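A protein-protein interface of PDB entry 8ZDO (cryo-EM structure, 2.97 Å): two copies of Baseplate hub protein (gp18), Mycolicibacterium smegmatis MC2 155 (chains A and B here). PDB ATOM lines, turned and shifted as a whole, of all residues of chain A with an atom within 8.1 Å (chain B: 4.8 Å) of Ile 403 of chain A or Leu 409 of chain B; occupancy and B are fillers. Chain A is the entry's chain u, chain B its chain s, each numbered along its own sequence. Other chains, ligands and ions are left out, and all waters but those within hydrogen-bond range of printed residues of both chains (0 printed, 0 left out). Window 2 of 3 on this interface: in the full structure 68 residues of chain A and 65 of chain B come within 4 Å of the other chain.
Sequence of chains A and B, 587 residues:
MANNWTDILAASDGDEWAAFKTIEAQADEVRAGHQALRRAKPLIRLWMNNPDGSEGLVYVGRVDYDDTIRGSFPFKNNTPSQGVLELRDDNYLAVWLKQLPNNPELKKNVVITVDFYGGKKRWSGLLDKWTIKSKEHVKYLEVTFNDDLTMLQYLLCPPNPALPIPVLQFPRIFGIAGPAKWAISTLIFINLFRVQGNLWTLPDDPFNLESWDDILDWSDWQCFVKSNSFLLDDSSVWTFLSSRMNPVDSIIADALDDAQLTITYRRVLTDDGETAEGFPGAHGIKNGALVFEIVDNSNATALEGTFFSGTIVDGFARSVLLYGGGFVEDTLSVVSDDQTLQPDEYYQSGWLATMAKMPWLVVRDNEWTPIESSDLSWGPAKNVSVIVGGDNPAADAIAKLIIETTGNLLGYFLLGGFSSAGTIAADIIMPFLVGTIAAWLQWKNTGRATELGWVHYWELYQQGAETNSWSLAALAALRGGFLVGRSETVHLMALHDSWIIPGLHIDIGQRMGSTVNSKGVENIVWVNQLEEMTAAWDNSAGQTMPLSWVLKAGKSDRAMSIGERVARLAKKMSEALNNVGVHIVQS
Ile 398 of chain A touches Pro 431 of chain B.
CB of Pro 431 of chain B touches CA of Ala 399 of chain A, 3.6 Å away.
Ala 399 of chain A touches Phe 432 of chain B.
Ile 402 of chain A touches Thr 405 of chain B.
CD1 of Leu 409 of chain B touches CG2 of Ile 403 of chain A, 3.99 Å away.
Ile 428 of chain B touches Ile 403 of chain A.
CE2 of Phe 432 of chain B touches CD1 of Ile 403 of chain A, at 3.5 Å.
CG2 of Thr 406 of chain A touches OG1 of Thr 406 of chain B, at 3.5 Å.
Phe 413 of chain B touches Leu 410 of chain A (CE2 to CD2, 3.96 Å).
Thr 406 of chain A touches its own counterpart, Thr 406 of chain B.
6 positions are printed for both chains.
Of the 15 printed residues of chain A, 6 touch a printed residue of chain B.
Hydrophobic or aromatic side chains of chain A within 4 Å of the printed part of chain B: Ile 398, Ala 399, Ile 402, Ile 403 and Leu 410.
Of the 13 printed residues of chain B, 7 touch a printed residue of chain A.
Printed residues of chain B that touch a printed residue of chain A: Thr 405, Thr 406, Leu 409, Phe 413, Ile 428, Pro 431 and Phe 432.
Hydrophobic or aromatic side chains of chain B that line the printed part of chain A: Leu 409, Phe 413, Pro 431 and Phe 432.
Among the printed residues, no Asp or Glu carboxylate lies within 4 Å of a Lys or Arg side-chain nitrogen of the other chain.
Of the printed residues of chain B, Ile 403 of chain A touches Leu 409, Ile 428 and Phe 432.
Of the printed residues of chain A, Leu 409 of chain B touches Ile 403.
Printed residues of chain A within 4 Å of Pro 431 of chain B: Ile 398 (3.8 Å) and Ala 399 (3.6 Å).
Of the printed residues of chain B, Ala 399 of chain A touches Pro 431 and Phe 432.
Printed residues of chain A within 4 Å of Thr 406 of chain B: Thr 406.
Leu 410 of chain B touches none of the printed residues of chain A.
The nearest printed residue of chain B that does not touch Ile 403 of chain A is Pro 431 of chain B (4.4 Å).
The backbone carbonyl oxygen of Ile 402 of chain A sits at hydrogen-bond distance from the side-chain hydroxyl of Thr 405 of chain A, 3.3 Å away.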
ATOM      1  N   ALA A 397     -19.861  21.343   7.575  1.00  0.00           N
ATOM      2  CA  ALA A 397     -20.140  21.756   6.208  1.00  0.00           C
ATOM      3  C   ALA A 397     -18.829  21.929   5.455  1.00  0.00           C
ATOM      4  O   ALA A 397     -17.785  22.206   6.048  1.00  0.00           O
ATOM      5  CB  ALA A 397     -20.938  23.059   6.188  1.00  0.00           C
ATOM      6  N   ILE A 398     -18.880  21.748   4.134  1.00  0.00           N
ATOM      7  CA  ILE A 398     -17.654  21.804   3.345  1.00  0.00           C
ATOM      8  C   ILE A 398     -17.038  23.198   3.396  1.00  0.00           C
ATOM      9  O   ILE A 398     -15.809  23.341   3.400  1.00  0.00           O
ATOM     10  CB  ILE A 398     -17.921  21.337   1.898  1.00  0.00           C
ATOM     11  CG1 ILE A 398     -16.604  21.052   1.178  1.00  0.00           C
ATOM     12  CG2 ILE A 398     -18.754  22.351   1.129  1.00  0.00           C
ATOM     13  CD1 ILE A 398     -15.960  19.751   1.586  1.00  0.00           C
ATOM     14  N   ALA A 399     -17.868  24.242   3.456  1.00  0.00           N
ATOM     15  CA  ALA A 399     -17.343  25.596   3.584  1.00  0.00           C
ATOM     16  C   ALA A 399     -16.554  25.758   4.874  1.00  0.00           C
ATOM     17  O   ALA A 399     -15.465  26.346   4.877  1.00  0.00           O
ATOM     18  CB  ALA A 399     -18.486  26.608   3.526  1.00  0.00           C
ATOM     19  N   LYS A 400     -17.090  25.242   5.980  1.00  0.00           N
ATOM     20  CA  LYS A 400     -16.356  25.251   7.239  1.00  0.00           C
ATOM     21  C   LYS A 400     -15.063  24.458   7.117  1.00  0.00           C
ATOM     22  O   LYS A 400     -13.975  24.979   7.389  1.00  0.00           O
ATOM     23  CB  LYS A 400     -17.241  24.685   8.350  1.00  0.00           C
ATOM     24  CG  LYS A 400     -16.809  25.057   9.751  1.00  0.00           C
ATOM     25  CD  LYS A 400     -17.949  24.892  10.740  1.00  0.00           C
ATOM     26  CE  LYS A 400     -19.180  25.653  10.290  1.00  0.00           C
ATOM     27  NZ  LYS A 400     -20.196  25.766  11.372  1.00  0.00           N
ATOM     28  N   LEU A 401     -15.164  23.214   6.635  1.00  0.00           N
ATOM     29  CA  LEU A 401     -14.012  22.325   6.532  1.00  0.00           C
ATOM     30  C   LEU A 401     -12.894  22.936   5.703  1.00  0.00           C
ATOM     31  O   LEU A 401     -11.718  22.646   5.941  1.00  0.00           O
ATOM     32  CB  LEU A 401     -14.426  20.993   5.912  1.00  0.00           C
ATOM     33  CG  LEU A 401     -15.423  20.103   6.645  1.00  0.00           C
ATOM     34  CD1 LEU A 401     -15.802  18.932   5.760  1.00  0.00           C
ATOM     35  CD2 LEU A 401     -14.846  19.627   7.960  1.00  0.00           C
ATOM     36  N   ILE A 402     -13.231  23.752   4.712  1.00  0.00           N
ATOM     37  CA  ILE A 402     -12.190  24.391   3.919  1.00  0.00           C
ATOM     38  C   ILE A 402     -11.685  25.648   4.615  1.00  0.00           C
ATOM     39  O   ILE A 402     -10.527  25.711   5.046  1.00  0.00           O
ATOM     40  CB  ILE A 402     -12.701  24.694   2.500  1.00  0.00           C
ATOM     41  CG1 ILE A 402     -13.020  23.390   1.771  1.00  0.00           C
ATOM     42  CG2 ILE A 402     -11.673  25.489   1.721  1.00  0.00           C
ATOM     43  CD1 ILE A 402     -13.633  23.586   0.415  1.00  0.00           C
ATOM     44  N   ILE A 403     -12.558  26.642   4.782  1.00  0.00           N
ATOM     45  CA  ILE A 403     -12.106  27.968   5.190  1.00  0.00           C
ATOM     46  C   ILE A 403     -11.597  27.958   6.626  1.00  0.00           C
ATOM     47  O   ILE A 403     -10.488  28.428   6.909  1.00  0.00           O
ATOM     48  CB  ILE A 403     -13.234  28.995   4.999  1.00  0.00           C
ATOM     49  CG1 ILE A 403     -13.741  28.958   3.559  1.00  0.00           C
ATOM     50  CG2 ILE A 403     -12.753  30.389   5.358  1.00  0.00           C
ATOM     51  CD1 ILE A 403     -14.728  30.041   3.231  1.00  0.00           C
ATOM     52  N   GLU A 404     -12.396  27.434   7.560  1.00  0.00           N
ATOM     53  CA  GLU A 404     -12.023  27.541   8.965  1.00  0.00           C
ATOM     54  C   GLU A 404     -10.800  26.692   9.272  1.00  0.00           C
ATOM     55  O   GLU A 404      -9.904  27.125  10.004  1.00  0.00           O
ATOM     56  CB  GLU A 404     -13.199  27.139   9.854  1.00  0.00           C
ATOM     57  CG  GLU A 404     -14.418  28.028   9.694  1.00  0.00           C
ATOM     58  CD  GLU A 404     -15.385  27.909  10.852  1.00  0.00           C
ATOM     59  OE1 GLU A 404     -15.038  27.244  11.850  1.00  0.00           O
ATOM     60  OE2 GLU A 404     -16.494  28.476  10.762  1.00  0.00           O
ATOM     61  N   THR A 405     -10.737  25.485   8.709  1.00  0.00           N
ATOM     62  CA  THR A 405      -9.586  24.627   8.955  1.00  0.00           C
ATOM     63  C   THR A 405      -8.329  25.183   8.302  1.00  0.00           C
ATOM     64  O   THR A 405      -7.242  25.097   8.880  1.00  0.00           O
ATOM     65  CB  THR A 405      -9.864  23.211   8.467  1.00  0.00           C
ATOM     66  OG1 THR A 405      -9.875  23.190   7.036  1.00  0.00           O
ATOM     67  CG2 THR A 405     -11.204  22.739   8.989  1.00  0.00           C
ATOM     68  N   THR A 406      -8.448  25.774   7.108  1.00  0.00           N
ATOM     69  CA  THR A 406      -7.282  26.392   6.491  1.00  0.00           C
ATOM     70  C   THR A 406      -6.788  27.572   7.315  1.00  0.00           C
ATOM     71  O   THR A 406      -5.578  27.743   7.502  1.00  0.00           O
ATOM     72  CB  THR A 406      -7.608  26.831   5.066  1.00  0.00           C
ATOM     73  OG1 THR A 406      -8.296  25.775   4.388  1.00  0.00           O
ATOM     74  CG2 THR A 406      -6.334  27.156   4.313  1.00  0.00           C
ATOM     75  N   GLY A 407      -7.705  28.392   7.828  1.00  0.00           N
ATOM     76  CA  GLY A 407      -7.293  29.504   8.667  1.00  0.00           C
ATOM     77  C   GLY A 407      -6.641  29.052   9.958  1.00  0.00           C
ATOM     78  O   GLY A 407      -5.626  29.611  10.382  1.00  0.00           O
ATOM     79  N   ASN A 408      -7.212  28.031  10.599  1.00  0.00           N
ATOM     80  CA  ASN A 408      -6.634  27.515  11.835  1.00  0.00           C
ATOM     81  C   ASN A 408      -5.260  26.905  11.592  1.00  0.00           C
ATOM     82  O   ASN A 408      -4.332  27.115  12.382  1.00  0.00           O
ATOM     83  CB  ASN A 408      -7.576  26.487  12.456  1.00  0.00           C
ATOM     84  CG  ASN A 408      -8.890  27.095  12.884  1.00  0.00           C
ATOM     85  OD1 ASN A 408      -8.939  28.236  13.336  1.00  0.00           O
ATOM     86  ND2 ASN A 408      -9.968  26.337  12.736  1.00  0.00           N
ATOM     87  N   LEU A 409      -5.112  26.148  10.503  1.00  0.00           N
ATOM     88  CA  LEU A 409      -3.818  25.565  10.177  1.00  0.00           C
ATOM     89  C   LEU A 409      -2.794  26.642   9.851  1.00  0.00           C
ATOM     90  O   LEU A 409      -1.629  26.528  10.239  1.00  0.00           O
ATOM     91  CB  LEU A 409      -3.960  24.586   9.013  1.00  0.00           C
ATOM     92  CG  LEU A 409      -4.384  23.166   9.391  1.00  0.00           C
ATOM     93  CD1 LEU A 409      -4.984  22.444   8.201  1.00  0.00           C
ATOM     94  CD2 LEU A 409      -3.210  22.391   9.952  1.00  0.00           C
ATOM     95  N   LEU A 410      -3.204  27.697   9.145  1.00  0.00           N
ATOM     96  CA  LEU A 410      -2.280  28.787   8.858  1.00  0.00           C
ATOM     97  C   LEU A 410      -1.856  29.505  10.131  1.00  0.00           C
ATOM     98  O   LEU A 410      -0.685  29.865  10.281  1.00  0.00           O
ATOM     99  CB  LEU A 410      -2.904  29.769   7.871  1.00  0.00           C
ATOM    100  CG  LEU A 410      -1.913  30.798   7.327  1.00  0.00           C
ATOM    101  CD1 LEU A 410      -0.802  30.109   6.555  1.00  0.00           C
ATOM    102  CD2 LEU A 410      -2.616  31.817   6.465  1.00  0.00           C
ATOM    103  N   MET A 430     -10.775  19.345  12.179  1.00  0.00           N
ATOM    104  CA  MET A 430     -12.188  19.270  11.817  1.00  0.00           C
ATOM    105  C   MET A 430     -12.473  18.341  10.641  1.00  0.00           C
ATOM    106  O   MET A 430     -13.466  17.596  10.716  1.00  0.00           O
ATOM    107  CB  MET A 430     -12.724  20.679  11.538  1.00  0.00           C
ATOM    108  CG  MET A 430     -14.234  20.746  11.411  1.00  0.00           C
ATOM    109  SD  MET A 430     -14.799  22.242  10.582  1.00  0.00           S
ATOM    110  CE  MET A 430     -13.855  23.488  11.453  1.00  0.00           C
ATOM    111  N   THR B 405      -9.950  28.210  -3.787  1.00  0.00           N
ATOM    112  CA  THR B 405     -10.389  28.918  -2.592  1.00  0.00           C
ATOM    113  C   THR B 405      -9.227  29.202  -1.656  1.00  0.00           C
ATOM    114  O   THR B 405      -9.123  30.307  -1.116  1.00  0.00           O
ATOM    115  CB  THR B 405     -11.467  28.126  -1.864  1.00  0.00           C
ATOM    116  OG1 THR B 405     -10.914  26.895  -1.385  1.00  0.00           O
ATOM    117  CG2 THR B 405     -12.608  27.833  -2.799  1.00  0.00           C
ATOM    118  N   THR B 406      -8.340  28.225  -1.443  1.00  0.00           N
ATOM    119  CA  THR B 406      -7.225  28.491  -0.544  1.00  0.00           C
ATOM    120  C   THR B 406      -6.241  29.480  -1.156  1.00  0.00           C
ATOM    121  O   THR B 406      -5.660  30.292  -0.431  1.00  0.00           O
ATOM    122  CB  THR B 406      -6.534  27.186  -0.139  1.00  0.00           C
ATOM    123  OG1 THR B 406      -5.626  27.442   0.939  1.00  0.00           O
ATOM    124  CG2 THR B 406      -5.770  26.575  -1.291  1.00  0.00           C
ATOM    125  N   GLY B 407      -6.078  29.473  -2.481  1.00  0.00           N
ATOM    126  CA  GLY B 407      -5.233  30.475  -3.108  1.00  0.00           C
ATOM    127  C   GLY B 407      -5.802  31.875  -2.990  1.00  0.00           C
ATOM    128  O   GLY B 407      -5.078  32.825  -2.675  1.00  0.00           O
ATOM    129  N   ASN B 408      -7.106  32.024  -3.230  1.00  0.00           N
ATOM    130  CA  ASN B 408      -7.745  33.328  -3.091  1.00  0.00           C
ATOM    131  C   ASN B 408      -7.711  33.807  -1.646  1.00  0.00           C
ATOM    132  O   ASN B 408      -7.482  34.992  -1.381  1.00  0.00           O
ATOM    133  CB  ASN B 408      -9.182  33.262  -3.600  1.00  0.00           C
ATOM    134  CG  ASN B 408      -9.260  32.946  -5.075  1.00  0.00           C
ATOM    135  OD1 ASN B 408      -8.325  33.211  -5.826  1.00  0.00           O
ATOM    136  ND2 ASN B 408     -10.378  32.373  -5.498  1.00  0.00           N
ATOM    137  N   LEU B 409      -7.942  32.898  -0.696  1.00  0.00           N
ATOM    138  CA  LEU B 409      -7.884  33.263   0.713  1.00  0.00           C
ATOM    139  C   LEU B 409      -6.479  33.685   1.113  1.00  0.00           C
ATOM    140  O   LEU B 409      -6.307  34.647   1.865  1.00  0.00           O
ATOM    141  CB  LEU B 409      -8.364  32.101   1.579  1.00  0.00           C
ATOM    142  CG  LEU B 409      -9.875  32.005   1.777  1.00  0.00           C
ATOM    143  CD1 LEU B 409     -10.267  30.617   2.247  1.00  0.00           C
ATOM    144  CD2 LEU B 409     -10.346  33.055   2.759  1.00  0.00           C
ATOM    145  N   LEU B 410      -5.456  32.980   0.623  1.00  0.00           N
ATOM    146  CA  LEU B 410      -4.087  33.375   0.925  1.00  0.00           C
ATOM    147  C   LEU B 410      -3.751  34.729   0.315  1.00  0.00           C
ATOM    148  O   LEU B 410      -3.068  35.541   0.944  1.00  0.00           O
ATOM    149  CB  LEU B 410      -3.106  32.313   0.441  1.00  0.00           C
ATOM    150  CG  LEU B 410      -1.706  32.454   1.039  1.00  0.00           C
ATOM    151  CD1 LEU B 410      -1.767  32.402   2.554  1.00  0.00           C
ATOM    152  CD2 LEU B 410      -0.783  31.385   0.508  1.00  0.00           C
ATOM    153  N   GLY B 411      -4.211  34.989  -0.909  1.00  0.00           N
ATOM    154  CA  GLY B 411      -3.986  36.299  -1.503  1.00  0.00           C
ATOM    155  C   GLY B 411      -4.650  37.413  -0.717  1.00  0.00           C
ATOM    156  O   GLY B 411      -4.040  38.455  -0.459  1.00  0.00           O
ATOM    157  N   TYR B 412      -5.904  37.200  -0.312  1.00  0.00           N
ATOM    158  CA  TYR B 412      -6.615  38.176   0.507  1.00  0.00           C
ATOM    159  C   TYR B 412      -5.907  38.397   1.838  1.00  0.00           C
ATOM    160  O   TYR B 412      -5.752  39.537   2.290  1.00  0.00           O
ATOM    161  CB  TYR B 412      -8.047  37.688   0.724  1.00  0.00           C
ATOM    162  CG  TYR B 412      -9.003  38.688   1.322  1.00  0.00           C
ATOM    163  CD1 TYR B 412      -9.313  39.865   0.662  1.00  0.00           C
ATOM    164  CD2 TYR B 412      -9.625  38.436   2.536  1.00  0.00           C
ATOM    165  CE1 TYR B 412     -10.197  40.773   1.203  1.00  0.00           C
ATOM    166  CE2 TYR B 412     -10.510  39.336   3.084  1.00  0.00           C
ATOM    167  CZ  TYR B 412     -10.792  40.503   2.412  1.00  0.00           C
ATOM    168  OH  TYR B 412     -11.673  41.408   2.954  1.00  0.00           O
ATOM    169  N   PHE B 413      -5.458  37.311   2.469  1.00  0.00           N
ATOM    170  CA  PHE B 413      -4.752  37.394   3.741  1.00  0.00           C
ATOM    171  C   PHE B 413      -3.448  38.173   3.606  1.00  0.00           C
ATOM    172  O   PHE B 413      -3.131  39.022   4.444  1.00  0.00           O
ATOM    173  CB  PHE B 413      -4.508  35.974   4.259  1.00  0.00           C
ATOM    174  CG  PHE B 413      -3.380  35.853   5.234  1.00  0.00           C
ATOM    175  CD1 PHE B 413      -3.589  36.030   6.585  1.00  0.00           C
ATOM    176  CD2 PHE B 413      -2.111  35.511   4.801  1.00  0.00           C
ATOM    177  CE1 PHE B 413      -2.550  35.901   7.476  1.00  0.00           C
ATOM    178  CE2 PHE B 413      -1.073  35.385   5.688  1.00  0.00           C
ATOM    179  CZ  PHE B 413      -1.294  35.580   7.027  1.00  0.00           C
ATOM    180  N   PHE B 418      -8.174  40.360   6.151  1.00  0.00           N
ATOM    181  CA  PHE B 418      -8.637  39.983   7.481  1.00  0.00           C
ATOM    182  C   PHE B 418      -8.155  40.964   8.540  1.00  0.00           C
ATOM    183  O   PHE B 418      -8.805  41.120   9.579  1.00  0.00           O
ATOM    184  CB  PHE B 418      -8.184  38.563   7.802  1.00  0.00           C
ATOM    185  CG  PHE B 418      -8.731  37.536   6.860  1.00  0.00           C
ATOM    186  CD1 PHE B 418     -10.051  37.135   6.947  1.00  0.00           C
ATOM    187  CD2 PHE B 418      -7.931  36.981   5.878  1.00  0.00           C
ATOM    188  CE1 PHE B 418     -10.559  36.196   6.077  1.00  0.00           C
ATOM    189  CE2 PHE B 418      -8.434  36.042   5.008  1.00  0.00           C
ATOM    190  CZ  PHE B 418      -9.748  35.648   5.107  1.00  0.00           C
ATOM    191  N   ILE B 428     -13.748  34.143  -2.600  1.00  0.00           N
ATOM    192  CA  ILE B 428     -13.349  33.394  -1.417  1.00  0.00           C
ATOM    193  C   ILE B 428     -14.544  32.738  -0.742  1.00  0.00           C
ATOM    194  O   ILE B 428     -14.435  32.291   0.405  1.00  0.00           O
ATOM    195  CB  ILE B 428     -12.587  34.284  -0.423  1.00  0.00           C
ATOM    196  CG1 ILE B 428     -13.498  35.393   0.100  1.00  0.00           C
ATOM    197  CG2 ILE B 428     -11.361  34.882  -1.081  1.00  0.00           C
ATOM    198  CD1 ILE B 428     -12.837  36.297   1.108  1.00  0.00           C
ATOM    199  N   PRO B 431     -17.067  27.919  -1.591  1.00  0.00           N
ATOM    200  CA  PRO B 431     -17.462  26.786  -0.738  1.00  0.00           C
ATOM    201  C   PRO B 431     -18.849  26.945  -0.141  1.00  0.00           C
ATOM    202  O   PRO B 431     -19.513  25.938   0.135  1.00  0.00           O
ATOM    203  CB  PRO B 431     -16.378  26.769   0.346  1.00  0.00           C
ATOM    204  CG  PRO B 431     -15.206  27.325  -0.305  1.00  0.00           C
ATOM    205  CD  PRO B 431     -15.704  28.372  -1.255  1.00  0.00           C
ATOM    206  N   PHE B 432     -19.307  28.178   0.076  1.00  0.00           N
ATOM    207  CA  PHE B 432     -20.660  28.407   0.564  1.00  0.00           C
ATOM    208  C   PHE B 432     -21.716  28.238  -0.520  1.00  0.00           C
ATOM    209  O   PHE B 432     -22.897  28.086  -0.194  1.00  0.00           O
ATOM    210  CB  PHE B 432     -20.777  29.810   1.157  1.00  0.00           C
ATOM    211  CG  PHE B 432     -20.040  29.987   2.447  1.00  0.00           C
ATOM    212  CD1 PHE B 432     -20.566  29.503   3.630  1.00  0.00           C
ATOM    213  CD2 PHE B 432     -18.823  30.639   2.478  1.00  0.00           C
ATOM    214  CE1 PHE B 432     -19.890  29.665   4.817  1.00  0.00           C
ATOM    215  CE2 PHE B 432     -18.143  30.803   3.662  1.00  0.00           C
ATOM    216  CZ  PHE B 432     -18.677  30.316   4.834  1.00  0.00           C
